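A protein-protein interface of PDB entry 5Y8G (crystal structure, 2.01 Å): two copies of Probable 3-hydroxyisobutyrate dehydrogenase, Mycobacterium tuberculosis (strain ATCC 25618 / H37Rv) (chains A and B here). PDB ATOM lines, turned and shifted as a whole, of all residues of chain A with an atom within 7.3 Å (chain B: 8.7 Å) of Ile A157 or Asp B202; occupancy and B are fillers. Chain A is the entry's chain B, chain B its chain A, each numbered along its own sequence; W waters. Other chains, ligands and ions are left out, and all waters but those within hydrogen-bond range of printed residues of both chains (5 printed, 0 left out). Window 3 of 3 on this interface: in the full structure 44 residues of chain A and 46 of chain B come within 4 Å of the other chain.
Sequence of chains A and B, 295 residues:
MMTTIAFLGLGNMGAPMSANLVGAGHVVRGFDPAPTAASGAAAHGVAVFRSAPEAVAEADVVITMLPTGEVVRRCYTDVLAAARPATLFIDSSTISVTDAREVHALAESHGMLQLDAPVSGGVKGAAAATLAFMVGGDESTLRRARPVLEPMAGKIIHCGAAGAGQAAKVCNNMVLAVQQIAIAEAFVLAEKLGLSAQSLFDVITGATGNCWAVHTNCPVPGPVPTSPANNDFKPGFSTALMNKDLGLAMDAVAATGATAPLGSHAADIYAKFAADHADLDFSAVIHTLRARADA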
ATOM      1  N   ASP A 116     -27.529 -15.896 -12.717  1.00  0.00           N
ATOM      2  CA  ASP A 116     -26.557 -15.950 -13.791  1.00  0.00           C
ATOM      3  C   ASP A 116     -27.126 -16.820 -14.906  1.00  0.00           C
ATOM      4  O   ASP A 116     -27.571 -17.922 -14.647  1.00  0.00           O
ATOM      5  CB  ASP A 116     -25.170 -16.435 -13.378  1.00  0.00           C
ATOM      6  CG  ASP A 116     -25.167 -17.749 -12.616  1.00  0.00           C
ATOM      7  OD1 ASP A 116     -24.534 -18.755 -13.076  1.00  0.00           O
ATOM      8  OD2 ASP A 116     -25.719 -17.734 -11.485  1.00  0.00           O
ATOM      9  N   ALA A 132     -28.613 -21.469 -25.962  1.00  0.00           N
ATOM     10  CA  ALA A 132     -28.776 -22.225 -24.717  1.00  0.00           C
ATOM     11  C   ALA A 132     -28.421 -21.369 -23.536  1.00  0.00           C
ATOM     12  O   ALA A 132     -27.300 -20.866 -23.494  1.00  0.00           O
ATOM     13  CB  ALA A 132     -27.918 -23.461 -24.754  1.00  0.00           C
ATOM     14  N   PHE A 133     -29.344 -21.209 -22.606  1.00  0.00           N
ATOM     15  CA  PHE A 133     -29.110 -20.494 -21.331  1.00  0.00           C
ATOM     16  C   PHE A 133     -28.835 -21.516 -20.237  1.00  0.00           C
ATOM     17  O   PHE A 133     -29.602 -22.445 -20.045  1.00  0.00           O
ATOM     18  CB  PHE A 133     -30.325 -19.681 -20.895  1.00  0.00           C
ATOM     19  CG  PHE A 133     -30.605 -18.438 -21.749  1.00  0.00           C
ATOM     20  CD1 PHE A 133     -30.241 -17.161 -21.300  1.00  0.00           C
ATOM     21  CD2 PHE A 133     -31.225 -18.527 -22.957  1.00  0.00           C
ATOM     22  CE1 PHE A 133     -30.458 -16.029 -22.073  1.00  0.00           C
ATOM     23  CE2 PHE A 133     -31.491 -17.377 -23.739  1.00  0.00           C
ATOM     24  CZ  PHE A 133     -31.087 -16.127 -23.279  1.00  0.00           C
ATOM     25  N   MET A 134     -27.724 -21.345 -19.555  1.00  0.00           N
ATOM     26  CA  MET A 134     -27.330 -22.207 -18.435  1.00  0.00           C
ATOM     27  C   MET A 134     -27.441 -21.373 -17.198  1.00  0.00           C
ATOM     28  O   MET A 134     -26.736 -20.397 -17.074  1.00  0.00           O
ATOM     29  CB  MET A 134     -25.919 -22.681 -18.672  1.00  0.00           C
ATOM     30  CG  MET A 134     -25.889 -23.662 -19.861  1.00  0.00           C
ATOM     31  SD  MET A 134     -24.252 -23.731 -20.618  1.00  0.00           S
ATOM     32  CE  MET A 134     -24.269 -22.232 -21.700  1.00  0.00           C
ATOM     33  N   VAL A 135     -28.368 -21.716 -16.311  1.00  0.00           N
ATOM     34  CA  VAL A 135     -28.865 -20.798 -15.283  1.00  0.00           C
ATOM     35  C   VAL A 135     -28.451 -21.241 -13.915  1.00  0.00           C
ATOM     36  O   VAL A 135     -28.557 -22.433 -13.571  1.00  0.00           O
ATOM     37  CB  VAL A 135     -30.383 -20.739 -15.320  1.00  0.00           C
ATOM     38  CG1 VAL A 135     -30.915 -19.832 -14.206  1.00  0.00           C
ATOM     39  CG2 VAL A 135     -30.817 -20.186 -16.671  1.00  0.00           C
ATOM     40  N   GLY A 136     -27.980 -20.283 -13.132  1.00  0.00           N
ATOM     41  CA  GLY A 136     -27.708 -20.454 -11.740  1.00  0.00           C
ATOM     42  C   GLY A 136     -28.579 -19.520 -10.911  1.00  0.00           C
ATOM     43  O   GLY A 136     -28.767 -18.364 -11.291  1.00  0.00           O
ATOM     44  N   LEU A 142     -36.070 -18.477 -11.492  1.00  0.00           N
ATOM     45  CA  LEU A 142     -36.041 -18.922 -12.869  1.00  0.00           C
ATOM     46  C   LEU A 142     -37.474 -19.092 -13.419  1.00  0.00           C
ATOM     47  O   LEU A 142     -37.732 -18.841 -14.573  1.00  0.00           O
ATOM     48  CB  LEU A 142     -35.258 -20.239 -12.966  1.00  0.00           C
ATOM     49  CG  LEU A 142     -35.251 -20.869 -14.339  1.00  0.00           C
ATOM     50  CD1 LEU A 142     -34.878 -19.934 -15.489  1.00  0.00           C
ATOM     51  CD2 LEU A 142     -34.376 -22.092 -14.346  1.00  0.00           C
ATOM     52  N   ARG A 146     -38.593 -17.304 -16.826  1.00  0.00           N
ATOM     53  CA  ARG A 146     -38.848 -18.122 -18.021  1.00  0.00           C
ATOM     54  C   ARG A 146     -39.547 -17.425 -19.186  1.00  0.00           C
ATOM     55  O   ARG A 146     -39.035 -17.422 -20.299  1.00  0.00           O
ATOM     56  CB  ARG A 146     -39.580 -19.411 -17.620  1.00  0.00           C
ATOM     57  CG  ARG A 146     -39.107 -20.608 -18.349  1.00  0.00           C
ATOM     58  CD  ARG A 146     -39.384 -21.881 -17.597  1.00  0.00           C
ATOM     59  NE  ARG A 146     -38.376 -22.841 -18.061  1.00  0.00           N
ATOM     60  CZ  ARG A 146     -37.568 -23.531 -17.272  1.00  0.00           C
ATOM     61  NH1 ARG A 146     -37.657 -23.416 -15.944  1.00  0.00           N
ATOM     62  NH2 ARG A 146     -36.680 -24.373 -17.813  1.00  0.00           N
ATOM     63  N   LEU A 149     -36.879 -15.277 -20.946  1.00  0.00           N
ATOM     64  CA  LEU A 149     -35.826 -16.069 -21.593  1.00  0.00           C
ATOM     65  C   LEU A 149     -36.320 -16.820 -22.825  1.00  0.00           C
ATOM     66  O   LEU A 149     -35.602 -16.939 -23.822  1.00  0.00           O
ATOM     67  CB  LEU A 149     -35.200 -17.051 -20.576  1.00  0.00           C
ATOM     68  CG  LEU A 149     -34.534 -16.456 -19.339  1.00  0.00           C
ATOM     69  CD1 LEU A 149     -33.938 -17.580 -18.550  1.00  0.00           C
ATOM     70  CD2 LEU A 149     -33.393 -15.491 -19.729  1.00  0.00           C
ATOM     71  N   LYS A 155     -32.857 -23.539 -25.552  1.00  0.00           N
ATOM     72  CA  LYS A 155     -32.739 -24.394 -24.340  1.00  0.00           C
ATOM     73  C   LYS A 155     -32.498 -23.506 -23.103  1.00  0.00           C
ATOM     74  O   LYS A 155     -31.747 -22.520 -23.157  1.00  0.00           O
ATOM     75  CB  LYS A 155     -31.545 -25.366 -24.471  1.00  0.00           C
ATOM     76  CG  LYS A 155     -31.660 -26.581 -23.594  1.00  0.00           C
ATOM     77  CD  LYS A 155     -30.501 -27.593 -23.721  1.00  0.00           C
ATOM     78  CE  LYS A 155     -30.093 -27.883 -25.166  1.00  0.00           C
ATOM     79  NZ  LYS A 155     -29.389 -29.200 -25.382  1.00  0.00           N
ATOM     80  N   ILE A 156     -33.152 -23.884 -22.012  1.00  0.00           N
ATOM     81  CA  ILE A 156     -32.960 -23.247 -20.717  1.00  0.00           C
ATOM     82  C   ILE A 156     -32.692 -24.380 -19.798  1.00  0.00           C
ATOM     83  O   ILE A 156     -33.510 -25.296 -19.680  1.00  0.00           O
ATOM     84  CB  ILE A 156     -34.208 -22.471 -20.294  1.00  0.00           C
ATOM     85  CG1 ILE A 156     -34.515 -21.342 -21.330  1.00  0.00           C
ATOM     86  CG2 ILE A 156     -34.047 -21.933 -18.885  1.00  0.00           C
ATOM     87  CD1 ILE A 156     -35.931 -20.725 -21.186  1.00  0.00           C
ATOM     88  N   ILE A 157     -31.546 -24.374 -19.166  1.00  0.00           N
ATOM     89  CA  ILE A 157     -31.294 -25.455 -18.201  1.00  0.00           C
ATOM     90  C   ILE A 157     -30.872 -24.904 -16.899  1.00  0.00           C
ATOM     91  O   ILE A 157     -30.003 -24.053 -16.837  1.00  0.00           O
ATOM     92  CB  ILE A 157     -30.351 -26.518 -18.794  1.00  0.00           C
ATOM     93  CG1 ILE A 157     -29.760 -27.426 -17.719  1.00  0.00           C
ATOM     94  CG2 ILE A 157     -29.197 -25.950 -19.581  1.00  0.00           C
ATOM     95  CD1 ILE A 157     -29.242 -28.724 -18.290  1.00  0.00           C
ATOM     96  N   HIS A 158     -31.522 -25.329 -15.837  1.00  0.00           N
ATOM     97  CA  HIS A 158     -31.192 -24.901 -14.501  1.00  0.00           C
ATOM     98  C   HIS A 158     -30.016 -25.732 -13.964  1.00  0.00           C
ATOM     99  O   HIS A 158     -30.131 -26.972 -13.801  1.00  0.00           O
ATOM    100  CB  HIS A 158     -32.378 -25.056 -13.543  1.00  0.00           C
ATOM    101  CG  HIS A 158     -32.135 -24.424 -12.210  1.00  0.00           C
ATOM    102  ND1 HIS A 158     -32.781 -24.821 -11.073  1.00  0.00           N
ATOM    103  CD2 HIS A 158     -31.302 -23.430 -11.829  1.00  0.00           C
ATOM    104  CE1 HIS A 158     -32.367 -24.094 -10.046  1.00  0.00           C
ATOM    105  NE2 HIS A 158     -31.482 -23.225 -10.481  1.00  0.00           N
ATOM    106  N   CYS A 159     -28.915 -25.073 -13.650  1.00  0.00           N
ATOM    107  CA  CYS A 159     -27.687 -25.781 -13.320  1.00  0.00           C
ATOM    108  C   CYS A 159     -27.427 -25.926 -11.796  1.00  0.00           C
ATOM    109  O   CYS A 159     -26.549 -26.691 -11.406  1.00  0.00           O
ATOM    110  CB  CYS A 159     -26.507 -25.061 -13.964  1.00  0.00           C
ATOM    111  SG  CYS A 159     -26.550 -25.170 -15.732  1.00  0.00           S
ATOM    112  N   GLY A 160     -28.111 -25.166 -10.959  1.00  0.00           N
ATOM    113  CA  GLY A 160     -27.858 -25.179  -9.539  1.00  0.00           C
ATOM    114  C   GLY A 160     -27.966 -23.754  -8.979  1.00  0.00           C
ATOM    115  O   GLY A 160     -28.654 -22.876  -9.565  1.00  0.00           O
ATOM    116  N   GLY A 165     -24.455 -21.624 -13.414  1.00  0.00           N
ATOM    117  CA  GLY A 165     -24.547 -21.400 -14.819  1.00  0.00           C
ATOM    118  C   GLY A 165     -23.176 -21.214 -15.391  1.00  0.00           C
ATOM    119  O   GLY A 165     -22.798 -21.859 -16.360  1.00  0.00           O
ATOM    120  N   ALA A 168     -21.037 -24.410 -15.247  1.00  0.00           N
ATOM    121  CA  ALA A 168     -21.364 -25.419 -16.198  1.00  0.00           C
ATOM    122  C   ALA A 168     -20.792 -25.039 -17.592  1.00  0.00           C
ATOM    123  O   ALA A 168     -20.264 -25.897 -18.337  1.00  0.00           O
ATOM    124  CB  ALA A 168     -22.852 -25.562 -16.270  1.00  0.00           C
ATOM    125  N   PHE B 187     -15.484 -33.042 -14.217  1.00  0.00           N
ATOM    126  CA  PHE B 187     -16.223 -33.444 -13.045  1.00  0.00           C
ATOM    127  C   PHE B 187     -15.568 -33.029 -11.745  1.00  0.00           C
ATOM    128  O   PHE B 187     -16.261 -32.618 -10.796  1.00  0.00           O
ATOM    129  CB  PHE B 187     -16.563 -34.939 -13.013  1.00  0.00           C
ATOM    130  CG  PHE B 187     -17.725 -35.265 -13.878  1.00  0.00           C
ATOM    131  CD1 PHE B 187     -19.029 -35.113 -13.386  1.00  0.00           C
ATOM    132  CD2 PHE B 187     -17.526 -35.606 -15.220  1.00  0.00           C
ATOM    133  CE1 PHE B 187     -20.117 -35.338 -14.192  1.00  0.00           C
ATOM    134  CE2 PHE B 187     -18.615 -35.865 -16.030  1.00  0.00           C
ATOM    135  CZ  PHE B 187     -19.936 -35.726 -15.518  1.00  0.00           C
ATOM    136  N   LEU B 195     -20.959 -27.351  -8.222  1.00  0.00           N
ATOM    137  CA  LEU B 195     -21.885 -27.795  -9.275  1.00  0.00           C
ATOM    138  C   LEU B 195     -22.045 -29.296  -9.147  1.00  0.00           C
ATOM    139  O   LEU B 195     -21.030 -30.030  -9.223  1.00  0.00           O
ATOM    140  CB  LEU B 195     -21.297 -27.415 -10.657  1.00  0.00           C
ATOM    141  CG  LEU B 195     -21.919 -27.888 -11.953  1.00  0.00           C
ATOM    142  CD1 LEU B 195     -23.329 -27.377 -12.114  1.00  0.00           C
ATOM    143  CD2 LEU B 195     -21.080 -27.494 -13.177  1.00  0.00           C
ATOM    144  N   SER B 196     -23.277 -29.775  -8.978  1.00  0.00           N
ATOM    145  CA  SER B 196     -23.485 -31.224  -8.826  1.00  0.00           C
ATOM    146  C   SER B 196     -23.071 -32.047 -10.114  1.00  0.00           C
ATOM    147  O   SER B 196     -23.037 -31.555 -11.247  1.00  0.00           O
ATOM    148  CB  SER B 196     -24.926 -31.544  -8.437  1.00  0.00           C
ATOM    149  OG  SER B 196     -25.708 -31.464  -9.591  1.00  0.00           O
ATOM    150  N   ALA B 197     -22.777 -33.307  -9.891  1.00  0.00           N
ATOM    151  CA  ALA B 197     -22.338 -34.190 -10.938  1.00  0.00           C
ATOM    152  C   ALA B 197     -23.482 -34.414 -11.925  1.00  0.00           C
ATOM    153  O   ALA B 197     -23.270 -34.407 -13.122  1.00  0.00           O
ATOM    154  CB  ALA B 197     -21.846 -35.516 -10.297  1.00  0.00           C
ATOM    155  N   GLN B 198     -24.709 -34.564 -11.453  1.00  0.00           N
ATOM    156  CA  GLN B 198     -25.878 -34.763 -12.361  1.00  0.00           C
ATOM    157  C   GLN B 198     -26.102 -33.529 -13.229  1.00  0.00           C
ATOM    158  O   GLN B 198     -26.474 -33.632 -14.395  1.00  0.00           O
ATOM    159  CB  GLN B 198     -27.163 -35.083 -11.592  1.00  0.00           C
ATOM    160  CG  GLN B 198     -28.310 -35.466 -12.502  1.00  0.00           C
ATOM    161  CD  GLN B 198     -28.052 -36.780 -13.230  1.00  0.00           C
ATOM    162  OE1 GLN B 198     -27.652 -37.743 -12.602  1.00  0.00           O
ATOM    163  NE2 GLN B 198     -28.232 -36.809 -14.555  1.00  0.00           N
ATOM    164  N   SER B 199     -25.866 -32.362 -12.637  1.00  0.00           N
ATOM    165  CA  SER B 199     -26.089 -31.094 -13.326  1.00  0.00           C
ATOM    166  C   SER B 199     -25.060 -30.877 -14.420  1.00  0.00           C
ATOM    167  O   SER B 199     -25.406 -30.525 -15.521  1.00  0.00           O
ATOM    168  CB  SER B 199     -26.101 -29.951 -12.297  1.00  0.00           C
ATOM    169  OG  SER B 199     -26.219 -28.779 -13.100  1.00  0.00           O
ATOM    170  N   LEU B 200     -23.795 -31.156 -14.115  1.00  0.00           N
ATOM    171  CA  LEU B 200     -22.776 -31.093 -15.133  1.00  0.00           C
ATOM    172  C   LEU B 200     -23.032 -32.139 -16.206  1.00  0.00           C
ATOM    173  O   LEU B 200     -22.926 -31.829 -17.416  1.00  0.00           O
ATOM    174  CB  LEU B 200     -21.379 -31.270 -14.580  1.00  0.00           C
ATOM    175  CG  LEU B 200     -20.300 -31.298 -15.652  1.00  0.00           C
ATOM    176  CD1 LEU B 200     -20.222 -29.892 -16.288  1.00  0.00           C
ATOM    177  CD2 LEU B 200     -18.900 -31.783 -15.196  1.00  0.00           C
ATOM    178  N   PHE B 201     -23.355 -33.361 -15.792  1.00  0.00           N
ATOM    179  CA  PHE B 201     -23.686 -34.380 -16.767  1.00  0.00           C
ATOM    180  C   PHE B 201     -24.783 -33.950 -17.744  1.00  0.00           C
ATOM    181  O   PHE B 201     -24.614 -34.075 -18.942  1.00  0.00           O
ATOM    182  CB  PHE B 201     -24.136 -35.675 -16.054  1.00  0.00           C
ATOM    183  CG  PHE B 201     -24.526 -36.774 -17.015  1.00  0.00           C
ATOM    184  CD1 PHE B 201     -23.586 -37.679 -17.423  1.00  0.00           C
ATOM    185  CD2 PHE B 201     -25.824 -36.948 -17.438  1.00  0.00           C
ATOM    186  CE1 PHE B 201     -23.904 -38.702 -18.310  1.00  0.00           C
ATOM    187  CE2 PHE B 201     -26.180 -38.036 -18.288  1.00  0.00           C
ATOM    188  CZ  PHE B 201     -25.212 -38.916 -18.729  1.00  0.00           C
ATOM    189  N   ASP B 202     -25.901 -33.438 -17.229  1.00  0.00           N
ATOM    190  CA  ASP B 202     -27.041 -32.915 -18.050  1.00  0.00           C
ATOM    191  C   ASP B 202     -26.593 -31.823 -18.988  1.00  0.00           C
ATOM    192  O   ASP B 202     -27.042 -31.782 -20.089  1.00  0.00           O
ATOM    193  CB  ASP B 202     -28.196 -32.391 -17.199  1.00  0.00           C
ATOM    194  CG  ASP B 202     -28.867 -33.484 -16.347  1.00  0.00           C
ATOM    195  OD1 ASP B 202     -28.650 -34.678 -16.637  1.00  0.00           O
ATOM    196  OD2 ASP B 202     -29.551 -33.173 -15.339  1.00  0.00           O
ATOM    197  N   VAL B 203     -25.700 -30.922 -18.546  1.00  0.00           N
ATOM    198  CA  VAL B 203     -25.250 -29.868 -19.427  1.00  0.00           C
ATOM    199  C   VAL B 203     -24.371 -30.404 -20.523  1.00  0.00           C
ATOM    200  O   VAL B 203     -24.657 -30.217 -21.722  1.00  0.00           O
ATOM    201  CB  VAL B 203     -24.524 -28.730 -18.667  1.00  0.00           C
ATOM    202  CG1 VAL B 203     -23.978 -27.708 -19.688  1.00  0.00           C
ATOM    203  CG2 VAL B 203     -25.516 -28.054 -17.740  1.00  0.00           C
ATOM    204  N   ILE B 204     -23.288 -31.078 -20.124  1.00  0.00           N
ATOM    205  CA  ILE B 204     -22.284 -31.535 -21.128  1.00  0.00           C
ATOM    206  C   ILE B 204     -22.904 -32.499 -22.160  1.00  0.00           C
ATOM    207  O   ILE B 204     -22.669 -32.338 -23.369  1.00  0.00           O
ATOM    208  CB  ILE B 204     -21.081 -32.244 -20.544  1.00  0.00           C
ATOM    209  CG1 ILE B 204     -20.301 -31.285 -19.683  1.00  0.00           C
ATOM    210  CG2 ILE B 204     -20.115 -32.571 -21.671  1.00  0.00           C
ATOM    211  CD1 ILE B 204     -18.917 -31.811 -19.218  1.00  0.00           C
ATOM    212  N   THR B 205     -23.752 -33.421 -21.707  1.00  0.00           N
ATOM    213  CA  THR B 205     -24.362 -34.339 -22.672  1.00  0.00           C
ATOM    214  C   THR B 205     -25.308 -33.655 -23.650  1.00  0.00           C
ATOM    215  O   THR B 205     -25.478 -34.168 -24.723  1.00  0.00           O
ATOM    216  CB  THR B 205     -25.036 -35.569 -22.063  1.00  0.00           C
ATOM    217  OG1 THR B 205     -26.058 -35.143 -21.196  1.00  0.00           O
ATOM    218  CG2 THR B 205     -23.976 -36.420 -21.290  1.00  0.00           C
ATOM    219  N   GLY B 206     -25.903 -32.512 -23.277  1.00  0.00           N
ATOM    220  CA  GLY B 206     -26.687 -31.719 -24.220  1.00  0.00           C
ATOM    221  C   GLY B 206     -25.895 -30.646 -24.913  1.00  0.00           C
ATOM    222  O   GLY B 206     -26.459 -29.818 -25.568  1.00  0.00           O
ATOM    223  N   ALA B 207     -24.581 -30.584 -24.722  1.00  0.00           N
ATOM    224  CA  ALA B 207     -23.777 -29.483 -25.259  1.00  0.00           C
ATOM    225  C   ALA B 207     -22.576 -29.984 -26.100  1.00  0.00           C
ATOM    226  O   ALA B 207     -22.424 -31.196 -26.369  1.00  0.00           O
ATOM    227  CB  ALA B 207     -23.337 -28.592 -24.113  1.00  0.00           C
ATOM    228  N   ASN B 210     -20.057 -33.058 -25.334  1.00  0.00           N
ATOM    229  CA  ASN B 210     -20.502 -34.450 -25.223  1.00  0.00           C
ATOM    230  C   ASN B 210     -19.601 -35.458 -25.983  1.00  0.00           C
ATOM    231  O   ASN B 210     -19.165 -35.216 -27.129  1.00  0.00           O
ATOM    232  CB  ASN B 210     -21.907 -34.614 -25.762  1.00  0.00           C
ATOM    233  CG  ASN B 210     -22.550 -35.926 -25.328  1.00  0.00           C
ATOM    234  OD1 ASN B 210     -22.227 -36.488 -24.278  1.00  0.00           O
ATOM    235  ND2 ASN B 210     -23.481 -36.381 -26.106  1.00  0.00           N
ATOM    236  N   VAL B 214     -18.125 -39.366 -21.397  1.00  0.00           N
ATOM    237  CA  VAL B 214     -19.126 -38.968 -20.426  1.00  0.00           C
ATOM    238  C   VAL B 214     -20.472 -39.690 -20.587  1.00  0.00           C
ATOM    239  O   VAL B 214     -21.043 -40.153 -19.581  1.00  0.00           O
ATOM    240  CB  VAL B 214     -19.284 -37.401 -20.295  1.00  0.00           C
ATOM    241  CG1 VAL B 214     -19.567 -36.735 -21.620  1.00  0.00           C
ATOM    242  CG2 VAL B 214     -20.394 -37.050 -19.291  1.00  0.00           C
ATOM    243  N   CYS B 218     -19.063 -42.274 -17.898  1.00  0.00           N
ATOM    244  CA  CYS B 218     -19.054 -41.256 -16.830  1.00  0.00           C
ATOM    245  C   CYS B 218     -18.263 -41.720 -15.612  1.00  0.00           C
ATOM    246  O   CYS B 218     -18.657 -42.743 -14.980  1.00  0.00           O
ATOM    247  CB  CYS B 218     -20.479 -40.986 -16.406  1.00  0.00           C
ATOM    248  SG  CYS B 218     -20.596 -39.637 -15.245  1.00  0.00           S
ATOM    249  N   PRO B 223     -24.754 -40.723 -12.605  1.00  0.00           N
ATOM    250  CA  PRO B 223     -25.491 -40.298 -13.823  1.00  0.00           C
ATOM    251  C   PRO B 223     -25.695 -41.372 -14.901  1.00  0.00           C
ATOM    252  O   PRO B 223     -26.640 -41.276 -15.704  1.00  0.00           O
ATOM    253  CB  PRO B 223     -24.650 -39.141 -14.353  1.00  0.00           C
ATOM    254  CG  PRO B 223     -23.961 -38.589 -13.135  1.00  0.00           C
ATOM    255  CD  PRO B 223     -23.754 -39.731 -12.171  1.00  0.00           C
HETATM  256  O   HOH W   1     -26.748 -26.994 -24.856  1.00  0.00           O
HETATM  257  O   HOH W   2     -29.505 -29.123 -12.000  1.00  0.00           O
HETATM  258  O   HOH W   3     -28.971 -29.938 -22.283  1.00  0.00           O
HETATM  259  O   HOH W   4     -28.235 -29.010 -14.953  1.00  0.00           O
HETATM  260  O   HOH W   5     -25.596 -28.083  -9.150  1.00  0.00           O
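No position is printed for both chains.
OG of Ser B199 lies within hydrogen-bond range of O of Cys A159. The backbone carbonyl oxygen (O) of Gly B206 sits at hydrogen-bond distance from the side-chain amino group (NZ) of Lys A155, at 3.0 Å.
Of the 17 printed residues of chain A, 4 touch a printed residue of chain B. Of the 18 printed residues of chain B, 5 touch a printed residue of chain A. Hydrophobic or aromatic side chains of chain B that line the printed part of chain A: Leu B195 and Val B203. Among the printed residues, 8 pairs touch across the chains. Among the printed residues, no Asp or Glu carboxylate lies within 4 Å of a Lys or Arg side-chain nitrogen of the other chain.
Among the printed residues, merely in contact across the chains: Cys A159 with Leu B195 (3.4 Å), Cys A159 with Val B203 (3.7 Å), Ala A168 with Leu B195 (3.7 Å), Ile A157 with Val B203 (3.8 Å), Ala A168 with Val B203 (3.9 Å) and Ile A157 with Asp B202 (3.97 Å).
Water W4 lies within hydrogen-bond range of OG of Ser B199 (2.7 Å) and O of His A158 (3.0 Å). Water W5 lies within hydrogen-bond range of O of Cys A159 (2.8 Å) and N of Ser B196 (2.9 Å). Water W2 bridges O of His A158 (2.9 Å) and OG of Ser B199 (3.5 Å). Water W1 lies within hydrogen-bond range of O of Gly B206 (2.9 Å) and NZ of Lys A155 (3.5 Å). Water W3 lies within hydrogen-bond range of the side-chain amino group of Lys A155 (3.2 Å) and the backbone carbonyl oxygen of Asp B202 (3.5 Å).
The side-chain hydroxyl of Ser B196 sits close to the backbone NH of Ser B199, 3.2 Å away. NE2 of Gln B198 sits at hydrogen-bond distance from OD1 of Asp B202, at 3.0 Å. O of Lys A155 is in hydrogen-bond range of N of Phe A133 (2.8 Å). The backbone carbonyl oxygen (O) of Phe A133 is in hydrogen-bond range of the backbone NH (N) of Ile A157. The backbone NH of Val A135 sits at hydrogen-bond distance from the backbone carbonyl oxygen of Ile A157 (2.9 Å). The side-chain sulfur of Cys A159 is in hydrogen-bond range of the backbone carbonyl oxygen of Ile A157.
Phe A133 touches none of the printed residues of chain B. Ile A157 touches just these residues of chain B: Asp B202 and Val B203. Of the printed residues of chain B, Ala A168 touches Leu B195 (3.7 Å) and Val B203 (3.9 Å). Printed residues of chain A within 4 Å of Ser B199: Cys A159. Of chain A, only Ile A157 comes within 4 Å of Asp B202. The nearest printed residue of chain A that does not touch Gly B206 is Ala A132 (6.6 Å).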
